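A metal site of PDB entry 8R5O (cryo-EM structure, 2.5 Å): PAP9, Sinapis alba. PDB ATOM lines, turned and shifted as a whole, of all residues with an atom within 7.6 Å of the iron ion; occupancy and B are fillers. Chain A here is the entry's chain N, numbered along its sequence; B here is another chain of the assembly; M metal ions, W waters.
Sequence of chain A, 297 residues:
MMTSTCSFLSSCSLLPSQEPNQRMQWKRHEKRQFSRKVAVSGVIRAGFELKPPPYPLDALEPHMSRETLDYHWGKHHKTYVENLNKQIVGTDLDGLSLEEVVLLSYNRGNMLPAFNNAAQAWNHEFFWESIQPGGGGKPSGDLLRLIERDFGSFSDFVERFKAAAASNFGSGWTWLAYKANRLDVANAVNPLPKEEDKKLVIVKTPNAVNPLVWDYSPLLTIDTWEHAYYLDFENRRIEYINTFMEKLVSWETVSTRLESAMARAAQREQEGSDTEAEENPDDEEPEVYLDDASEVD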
ATOM      1  N   HIS A  72       8.931 -15.279  -4.139  1.00  0.00           N
ATOM      2  CA  HIS A  72       8.172 -15.226  -2.893  1.00  0.00           C
ATOM      3  C   HIS A  72       6.687 -15.442  -3.158  1.00  0.00           C
ATOM      4  O   HIS A  72       6.032 -16.241  -2.484  1.00  0.00           O
ATOM      5  CB  HIS A  72       8.415 -13.905  -2.181  1.00  0.00           C
ATOM      6  CG  HIS A  72       8.088 -13.933  -0.723  1.00  0.00           C
ATOM      7  ND1 HIS A  72       8.276 -12.852   0.105  1.00  0.00           N
ATOM      8  CD2 HIS A  72       7.589 -14.922   0.059  1.00  0.00           C
ATOM      9  CE1 HIS A  72       7.913 -13.165   1.336  1.00  0.00           C
ATOM     10  NE2 HIS A  72       7.489 -14.423   1.336  1.00  0.00           N
ATOM     11  N   TRP A  73       6.140 -14.739  -4.140  1.00  0.00           N
ATOM     12  CA  TRP A  73       4.722 -14.870  -4.458  1.00  0.00           C
ATOM     13  C   TRP A  73       4.465 -15.972  -5.490  1.00  0.00           C
ATOM     14  O   TRP A  73       3.572 -16.800  -5.305  1.00  0.00           O
ATOM     15  CB  TRP A  73       4.173 -13.531  -4.965  1.00  0.00           C
ATOM     16  CG  TRP A  73       2.744 -13.608  -5.408  1.00  0.00           C
ATOM     17  CD1 TRP A  73       1.640 -13.548  -4.610  1.00  0.00           C
ATOM     18  CD2 TRP A  73       2.266 -13.755  -6.748  1.00  0.00           C
ATOM     19  NE1 TRP A  73       0.508 -13.651  -5.375  1.00  0.00           N
ATOM     20  CE2 TRP A  73       0.862 -13.778  -6.691  1.00  0.00           C
ATOM     21  CE3 TRP A  73       2.898 -13.866  -7.991  1.00  0.00           C
ATOM     22  CZ2 TRP A  73       0.071 -13.907  -7.818  1.00  0.00           C
ATOM     23  CZ3 TRP A  73       2.106 -13.994  -9.119  1.00  0.00           C
ATOM     24  CH2 TRP A  73       0.710 -14.017  -9.021  1.00  0.00           C
ATOM     25  N   HIS A  76       6.636 -19.567  -3.569  1.00  0.00           N
ATOM     26  CA  HIS A  76       6.370 -19.936  -2.190  1.00  0.00           C
ATOM     27  C   HIS A  76       4.887 -19.783  -1.847  1.00  0.00           C
ATOM     28  O   HIS A  76       4.245 -20.732  -1.383  1.00  0.00           O
ATOM     29  CB  HIS A  76       7.225 -19.091  -1.241  1.00  0.00           C
ATOM     30  CG  HIS A  76       8.688 -19.382  -1.336  1.00  0.00           C
ATOM     31  ND1 HIS A  76       9.290 -20.418  -0.664  1.00  0.00           N
ATOM     32  CD2 HIS A  76       9.676 -18.762  -2.016  1.00  0.00           C
ATOM     33  CE1 HIS A  76      10.578 -20.433  -0.926  1.00  0.00           C
ATOM     34  NE2 HIS A  76      10.847 -19.437  -1.750  1.00  0.00           N
ATOM     35  N   HIS A  77       4.338 -18.591  -2.078  1.00  0.00           N
ATOM     36  CA  HIS A  77       2.930 -18.350  -1.765  1.00  0.00           C
ATOM     37  C   HIS A  77       2.014 -19.213  -2.629  1.00  0.00           C
ATOM     38  O   HIS A  77       1.000 -19.714  -2.146  1.00  0.00           O
ATOM     39  CB  HIS A  77       2.605 -16.869  -1.928  1.00  0.00           C
ATOM     40  CG  HIS A  77       1.280 -16.471  -1.348  1.00  0.00           C
ATOM     41  ND1 HIS A  77       0.760 -15.206  -1.494  1.00  0.00           N
ATOM     42  CD2 HIS A  77       0.376 -17.176  -0.625  1.00  0.00           C
ATOM     43  CE1 HIS A  77      -0.409 -15.144  -0.881  1.00  0.00           C
ATOM     44  NE2 HIS A  77      -0.665 -16.324  -0.356  1.00  0.00           N
ATOM     45  N   TYR A  80       1.838 -22.789  -1.245  1.00  0.00           N
ATOM     46  CA  TYR A  80       1.026 -22.894  -0.037  1.00  0.00           C
ATOM     47  C   TYR A  80      -0.454 -23.008  -0.366  1.00  0.00           C
ATOM     48  O   TYR A  80      -1.168 -23.809   0.249  1.00  0.00           O
ATOM     49  CB  TYR A  80       1.283 -21.682   0.866  1.00  0.00           C
ATOM     50  CG  TYR A  80       2.624 -21.691   1.559  1.00  0.00           C
ATOM     51  CD1 TYR A  80       3.130 -22.846   2.132  1.00  0.00           C
ATOM     52  CD2 TYR A  80       3.401 -20.540   1.614  1.00  0.00           C
ATOM     53  CE1 TYR A  80       4.355 -22.854   2.754  1.00  0.00           C
ATOM     54  CE2 TYR A  80       4.628 -20.540   2.230  1.00  0.00           C
ATOM     55  CZ  TYR A  80       5.105 -21.697   2.809  1.00  0.00           C
ATOM     56  OH  TYR A  80       6.332 -21.697   3.425  1.00  0.00           O
ATOM     57  N   GLN A 120       0.311 -20.203   6.513  1.00  0.00           N
ATOM     58  CA  GLN A 120       1.241 -19.511   5.628  1.00  0.00           C
ATOM     59  C   GLN A 120       0.516 -18.795   4.501  1.00  0.00           C
ATOM     60  O   GLN A 120       0.916 -17.692   4.106  1.00  0.00           O
ATOM     61  CB  GLN A 120       2.271 -20.489   5.070  1.00  0.00           C
ATOM     62  CG  GLN A 120       3.391 -20.847   6.032  1.00  0.00           C
ATOM     63  CD  GLN A 120       4.310 -19.674   6.332  1.00  0.00           C
ATOM     64  OE1 GLN A 120       4.004 -18.829   7.168  1.00  0.00           O
ATOM     65  NE2 GLN A 120       5.448 -19.638   5.655  1.00  0.00           N
ATOM     66  N   ASN A 123      -0.800 -15.753   6.046  1.00  0.00           N
ATOM     67  CA  ASN A 123       0.270 -14.839   6.422  1.00  0.00           C
ATOM     68  C   ASN A 123       0.779 -14.044   5.232  1.00  0.00           C
ATOM     69  O   ASN A 123       1.019 -12.839   5.338  1.00  0.00           O
ATOM     70  CB  ASN A 123       1.421 -15.613   7.070  1.00  0.00           C
ATOM     71  CG  ASN A 123       1.077 -16.121   8.453  1.00  0.00           C
ATOM     72  OD1 ASN A 123       0.189 -15.594   9.125  1.00  0.00           O
ATOM     73  ND2 ASN A 123       1.782 -17.150   8.890  1.00  0.00           N
ATOM     74  N   HIS A 124       0.970 -14.705   4.087  1.00  0.00           N
ATOM     75  CA  HIS A 124       1.525 -14.009   2.928  1.00  0.00           C
ATOM     76  C   HIS A 124       0.538 -13.024   2.337  1.00  0.00           C
ATOM     77  O   HIS A 124       0.915 -11.921   1.936  1.00  0.00           O
ATOM     78  CB  HIS A 124       1.984 -15.024   1.877  1.00  0.00           C
ATOM     79  CG  HIS A 124       3.259 -15.721   2.235  1.00  0.00           C
ATOM     80  ND1 HIS A 124       3.298 -16.835   3.044  1.00  0.00           N
ATOM     81  CD2 HIS A 124       4.547 -15.441   1.924  1.00  0.00           C
ATOM     82  CE1 HIS A 124       4.547 -17.225   3.197  1.00  0.00           C
ATOM     83  NE2 HIS A 124       5.325 -16.392   2.520  1.00  0.00           N
ATOM     84  N   PHE A 127       0.796 -10.227   4.414  1.00  0.00           N
ATOM     85  CA  PHE A 127       2.069  -9.554   4.202  1.00  0.00           C
ATOM     86  C   PHE A 127       2.045  -8.647   2.985  1.00  0.00           C
ATOM     87  O   PHE A 127       2.583  -7.539   3.013  1.00  0.00           O
ATOM     88  CB  PHE A 127       3.186 -10.604   4.080  1.00  0.00           C
ATOM     89  CG  PHE A 127       4.545 -10.004   3.836  1.00  0.00           C
ATOM     90  CD1 PHE A 127       5.117  -9.133   4.737  1.00  0.00           C
ATOM     91  CD2 PHE A 127       5.267 -10.351   2.704  1.00  0.00           C
ATOM     92  CE1 PHE A 127       6.370  -8.593   4.518  1.00  0.00           C
ATOM     93  CE2 PHE A 127       6.518  -9.826   2.478  1.00  0.00           C
ATOM     94  CZ  PHE A 127       7.069  -8.947   3.386  1.00  0.00           C
ATOM     95  N   TRP A 128       1.425  -9.107   1.883  1.00  0.00           N
ATOM     96  CA  TRP A 128       1.408  -8.281   0.674  1.00  0.00           C
ATOM     97  C   TRP A 128       0.578  -7.017   0.861  1.00  0.00           C
ATOM     98  O   TRP A 128       0.914  -5.980   0.288  1.00  0.00           O
ATOM     99  CB  TRP A 128       0.869  -9.091  -0.513  1.00  0.00           C
ATOM    100  CG  TRP A 128       1.625 -10.361  -0.805  1.00  0.00           C
ATOM    101  CD1 TRP A 128       1.089 -11.604  -0.984  1.00  0.00           C
ATOM    102  CD2 TRP A 128       3.043 -10.516  -0.946  1.00  0.00           C
ATOM    103  NE1 TRP A 128       2.083 -12.511  -1.222  1.00  0.00           N
ATOM    104  CE2 TRP A 128       3.292 -11.869  -1.205  1.00  0.00           C
ATOM    105  CE3 TRP A 128       4.128  -9.635  -0.878  1.00  0.00           C
ATOM    106  CZ2 TRP A 128       4.584 -12.372  -1.398  1.00  0.00           C
ATOM    107  CZ3 TRP A 128       5.397 -10.137  -1.060  1.00  0.00           C
ATOM    108  CH2 TRP A 128       5.618 -11.486  -1.319  1.00  0.00           C
ATOM    109  N   GLY A 172      10.134 -17.078  10.860  1.00  0.00           N
ATOM    110  CA  GLY A 172       9.019 -16.603  11.660  1.00  0.00           C
ATOM    111  C   GLY A 172       8.505 -15.268  11.159  1.00  0.00           C
ATOM    112  O   GLY A 172       8.919 -14.773  10.111  1.00  0.00           O
ATOM    113  N   TRP A 173       7.604 -14.697  11.948  1.00  0.00           N
ATOM    114  CA  TRP A 173       6.962 -13.429  11.639  1.00  0.00           C
ATOM    115  C   TRP A 173       6.954 -12.538  12.878  1.00  0.00           C
ATOM    116  O   TRP A 173       6.907 -13.039  14.010  1.00  0.00           O
ATOM    117  CB  TRP A 173       5.515 -13.629  11.150  1.00  0.00           C
ATOM    118  CG  TRP A 173       5.378 -14.527   9.968  1.00  0.00           C
ATOM    119  CD1 TRP A 173       5.495 -15.892   9.950  1.00  0.00           C
ATOM    120  CD2 TRP A 173       5.077 -14.143   8.625  1.00  0.00           C
ATOM    121  NE1 TRP A 173       5.296 -16.373   8.682  1.00  0.00           N
ATOM    122  CE2 TRP A 173       5.036 -15.317   7.846  1.00  0.00           C
ATOM    123  CE3 TRP A 173       4.837 -12.918   8.000  1.00  0.00           C
ATOM    124  CZ2 TRP A 173       4.778 -15.298   6.475  1.00  0.00           C
ATOM    125  CZ3 TRP A 173       4.571 -12.902   6.640  1.00  0.00           C
ATOM    126  CH2 TRP A 173       4.542 -14.090   5.901  1.00  0.00           C
ATOM    127  N   ASP A 223       7.714 -10.449   7.059  1.00  0.00           N
ATOM    128  CA  ASP A 223       8.153 -11.823   6.864  1.00  0.00           C
ATOM    129  C   ASP A 223       9.649 -11.917   7.120  1.00  0.00           C
ATOM    130  O   ASP A 223      10.446 -11.314   6.392  1.00  0.00           O
ATOM    131  CB  ASP A 223       7.806 -12.288   5.446  1.00  0.00           C
ATOM    132  CG  ASP A 223       7.933 -13.785   5.283  1.00  0.00           C
ATOM    133  OD1 ASP A 223       8.339 -14.467   6.236  1.00  0.00           O
ATOM    134  OD2 ASP A 223       7.609 -14.279   4.182  1.00  0.00           O
ATOM    135  N   THR A 224      10.028 -12.664   8.151  1.00  0.00           N
ATOM    136  CA  THR A 224      11.438 -12.865   8.476  1.00  0.00           C
ATOM    137  C   THR A 224      11.943 -14.238   8.079  1.00  0.00           C
ATOM    138  O   THR A 224      13.040 -14.631   8.479  1.00  0.00           O
ATOM    139  CB  THR A 224      11.691 -12.622   9.969  1.00  0.00           C
ATOM    140  OG1 THR A 224      10.649 -13.228  10.747  1.00  0.00           O
ATOM    141  CG2 THR A 224      11.743 -11.131  10.272  1.00  0.00           C
ATOM    142  N   TRP A 225      11.172 -14.987   7.286  1.00  0.00           N
ATOM    143  CA  TRP A 225      11.728 -16.135   6.599  1.00  0.00           C
ATOM    144  C   TRP A 225      12.831 -15.659   5.660  1.00  0.00           C
ATOM    145  O   TRP A 225      12.724 -14.599   5.045  1.00  0.00           O
ATOM    146  CB  TRP A 225      10.655 -16.883   5.810  1.00  0.00           C
ATOM    147  CG  TRP A 225       9.700 -17.701   6.642  1.00  0.00           C
ATOM    148  CD1 TRP A 225       8.864 -17.236   7.623  1.00  0.00           C
ATOM    149  CD2 TRP A 225       9.463 -19.107   6.544  1.00  0.00           C
ATOM    150  NE1 TRP A 225       8.139 -18.276   8.146  1.00  0.00           N
ATOM    151  CE2 TRP A 225       8.485 -19.430   7.498  1.00  0.00           C
ATOM    152  CE3 TRP A 225       9.988 -20.118   5.743  1.00  0.00           C
ATOM    153  CZ2 TRP A 225       8.024 -20.731   7.681  1.00  0.00           C
ATOM    154  CZ3 TRP A 225       9.537 -21.409   5.926  1.00  0.00           C
ATOM    155  CH2 TRP A 225       8.563 -21.708   6.881  1.00  0.00           C
ATOM    156  N   GLU A 226      13.900 -16.442   5.561  1.00  0.00           N
ATOM    157  CA  GLU A 226      15.062 -15.998   4.794  1.00  0.00           C
ATOM    158  C   GLU A 226      14.748 -15.821   3.314  1.00  0.00           C
ATOM    159  O   GLU A 226      15.385 -15.007   2.641  1.00  0.00           O
ATOM    160  CB  GLU A 226      16.225 -16.966   5.000  1.00  0.00           C
ATOM    161  CG  GLU A 226      16.867 -16.832   6.369  1.00  0.00           C
ATOM    162  CD  GLU A 226      17.969 -17.852   6.624  1.00  0.00           C
ATOM    163  OE1 GLU A 226      17.826 -19.001   6.169  1.00  0.00           O
ATOM    164  OE2 GLU A 226      18.965 -17.491   7.279  1.00  0.00           O
ATOM    165  N   HIS A 227      13.764 -16.558   2.792  1.00  0.00           N
ATOM    166  CA  HIS A 227      13.408 -16.414   1.380  1.00  0.00           C
ATOM    167  C   HIS A 227      12.815 -15.046   1.070  1.00  0.00           C
ATOM    168  O   HIS A 227      12.768 -14.659  -0.096  1.00  0.00           O
ATOM    169  CB  HIS A 227      12.438 -17.516   0.950  1.00  0.00           C
ATOM    170  CG  HIS A 227      11.112 -17.482   1.640  1.00  0.00           C
ATOM    171  ND1 HIS A 227      10.646 -18.526   2.402  1.00  0.00           N
ATOM    172  CD2 HIS A 227      10.133 -16.537   1.660  1.00  0.00           C
ATOM    173  CE1 HIS A 227       9.445 -18.223   2.875  1.00  0.00           C
ATOM    174  NE2 HIS A 227       9.114 -17.023   2.444  1.00  0.00           N
ATOM    175  N   ALA A 228      12.365 -14.311   2.085  1.00  0.00           N
ATOM    176  CA  ALA A 228      11.754 -12.998   1.853  1.00  0.00           C
ATOM    177  C   ALA A 228      12.782 -11.924   1.531  1.00  0.00           C
ATOM    178  O   ALA A 228      12.418 -10.921   0.917  1.00  0.00           O
ATOM    179  CB  ALA A 228      10.929 -12.585   3.075  1.00  0.00           C
ATOM    180  N   GLU B 214      17.258 -22.200   4.868  1.00  0.00           N
ATOM    181  CA  GLU B 214      17.127 -21.690   3.510  1.00  0.00           C
ATOM    182  C   GLU B 214      18.400 -21.011   3.026  1.00  0.00           C
ATOM    183  O   GLU B 214      18.672 -21.014   1.820  1.00  0.00           O
ATOM    184  CB  GLU B 214      15.932 -20.739   3.419  1.00  0.00           C
ATOM    185  CG  GLU B 214      14.599 -21.453   3.270  1.00  0.00           C
ATOM    186  CD  GLU B 214      13.418 -20.507   3.231  1.00  0.00           C
ATOM    187  OE1 GLU B 214      13.479 -19.448   3.895  1.00  0.00           O
ATOM    188  OE2 GLU B 214      12.424 -20.822   2.555  1.00  0.00           O
HETATM  189 FE    FE M   1       7.466 -15.963   2.997  1.00  0.00          FE
HETATM  190  O   HOH W   1       7.298 -16.934   5.024  1.00  0.00           O
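OD1 of Asp 223 lies within hydrogen-bond range of N of Trp 225 (3.1 Å). O of His 72 sits at hydrogen-bond distance from N of His 77 (2.9 Å). O of His 124 sits close to NE1 of Trp 128 (3.4 Å). The side-chain carboxylate (OE2) of Glu 214 of chain B lies within hydrogen-bond range of a ring nitrogen (ND1) of His 227 (2.9 Å). O of Gln 120 is in hydrogen-bond range of ND1 of His 124.
The iron ion is bound by a ring nitrogen (NE2) of His 227, the side-chain carboxylate of Asp 223, a ring nitrogen (NE2) of His 124, water W1 and a ring nitrogen (NE2) of His 72. The iron ion has five donor atoms within binding distance.
Water W1 lies within hydrogen-bond range of the side-chain carboxylate of Asp 223 (2.9 Å) and the side-chain amide nitrogen of Gln 120 (3.3 Å).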
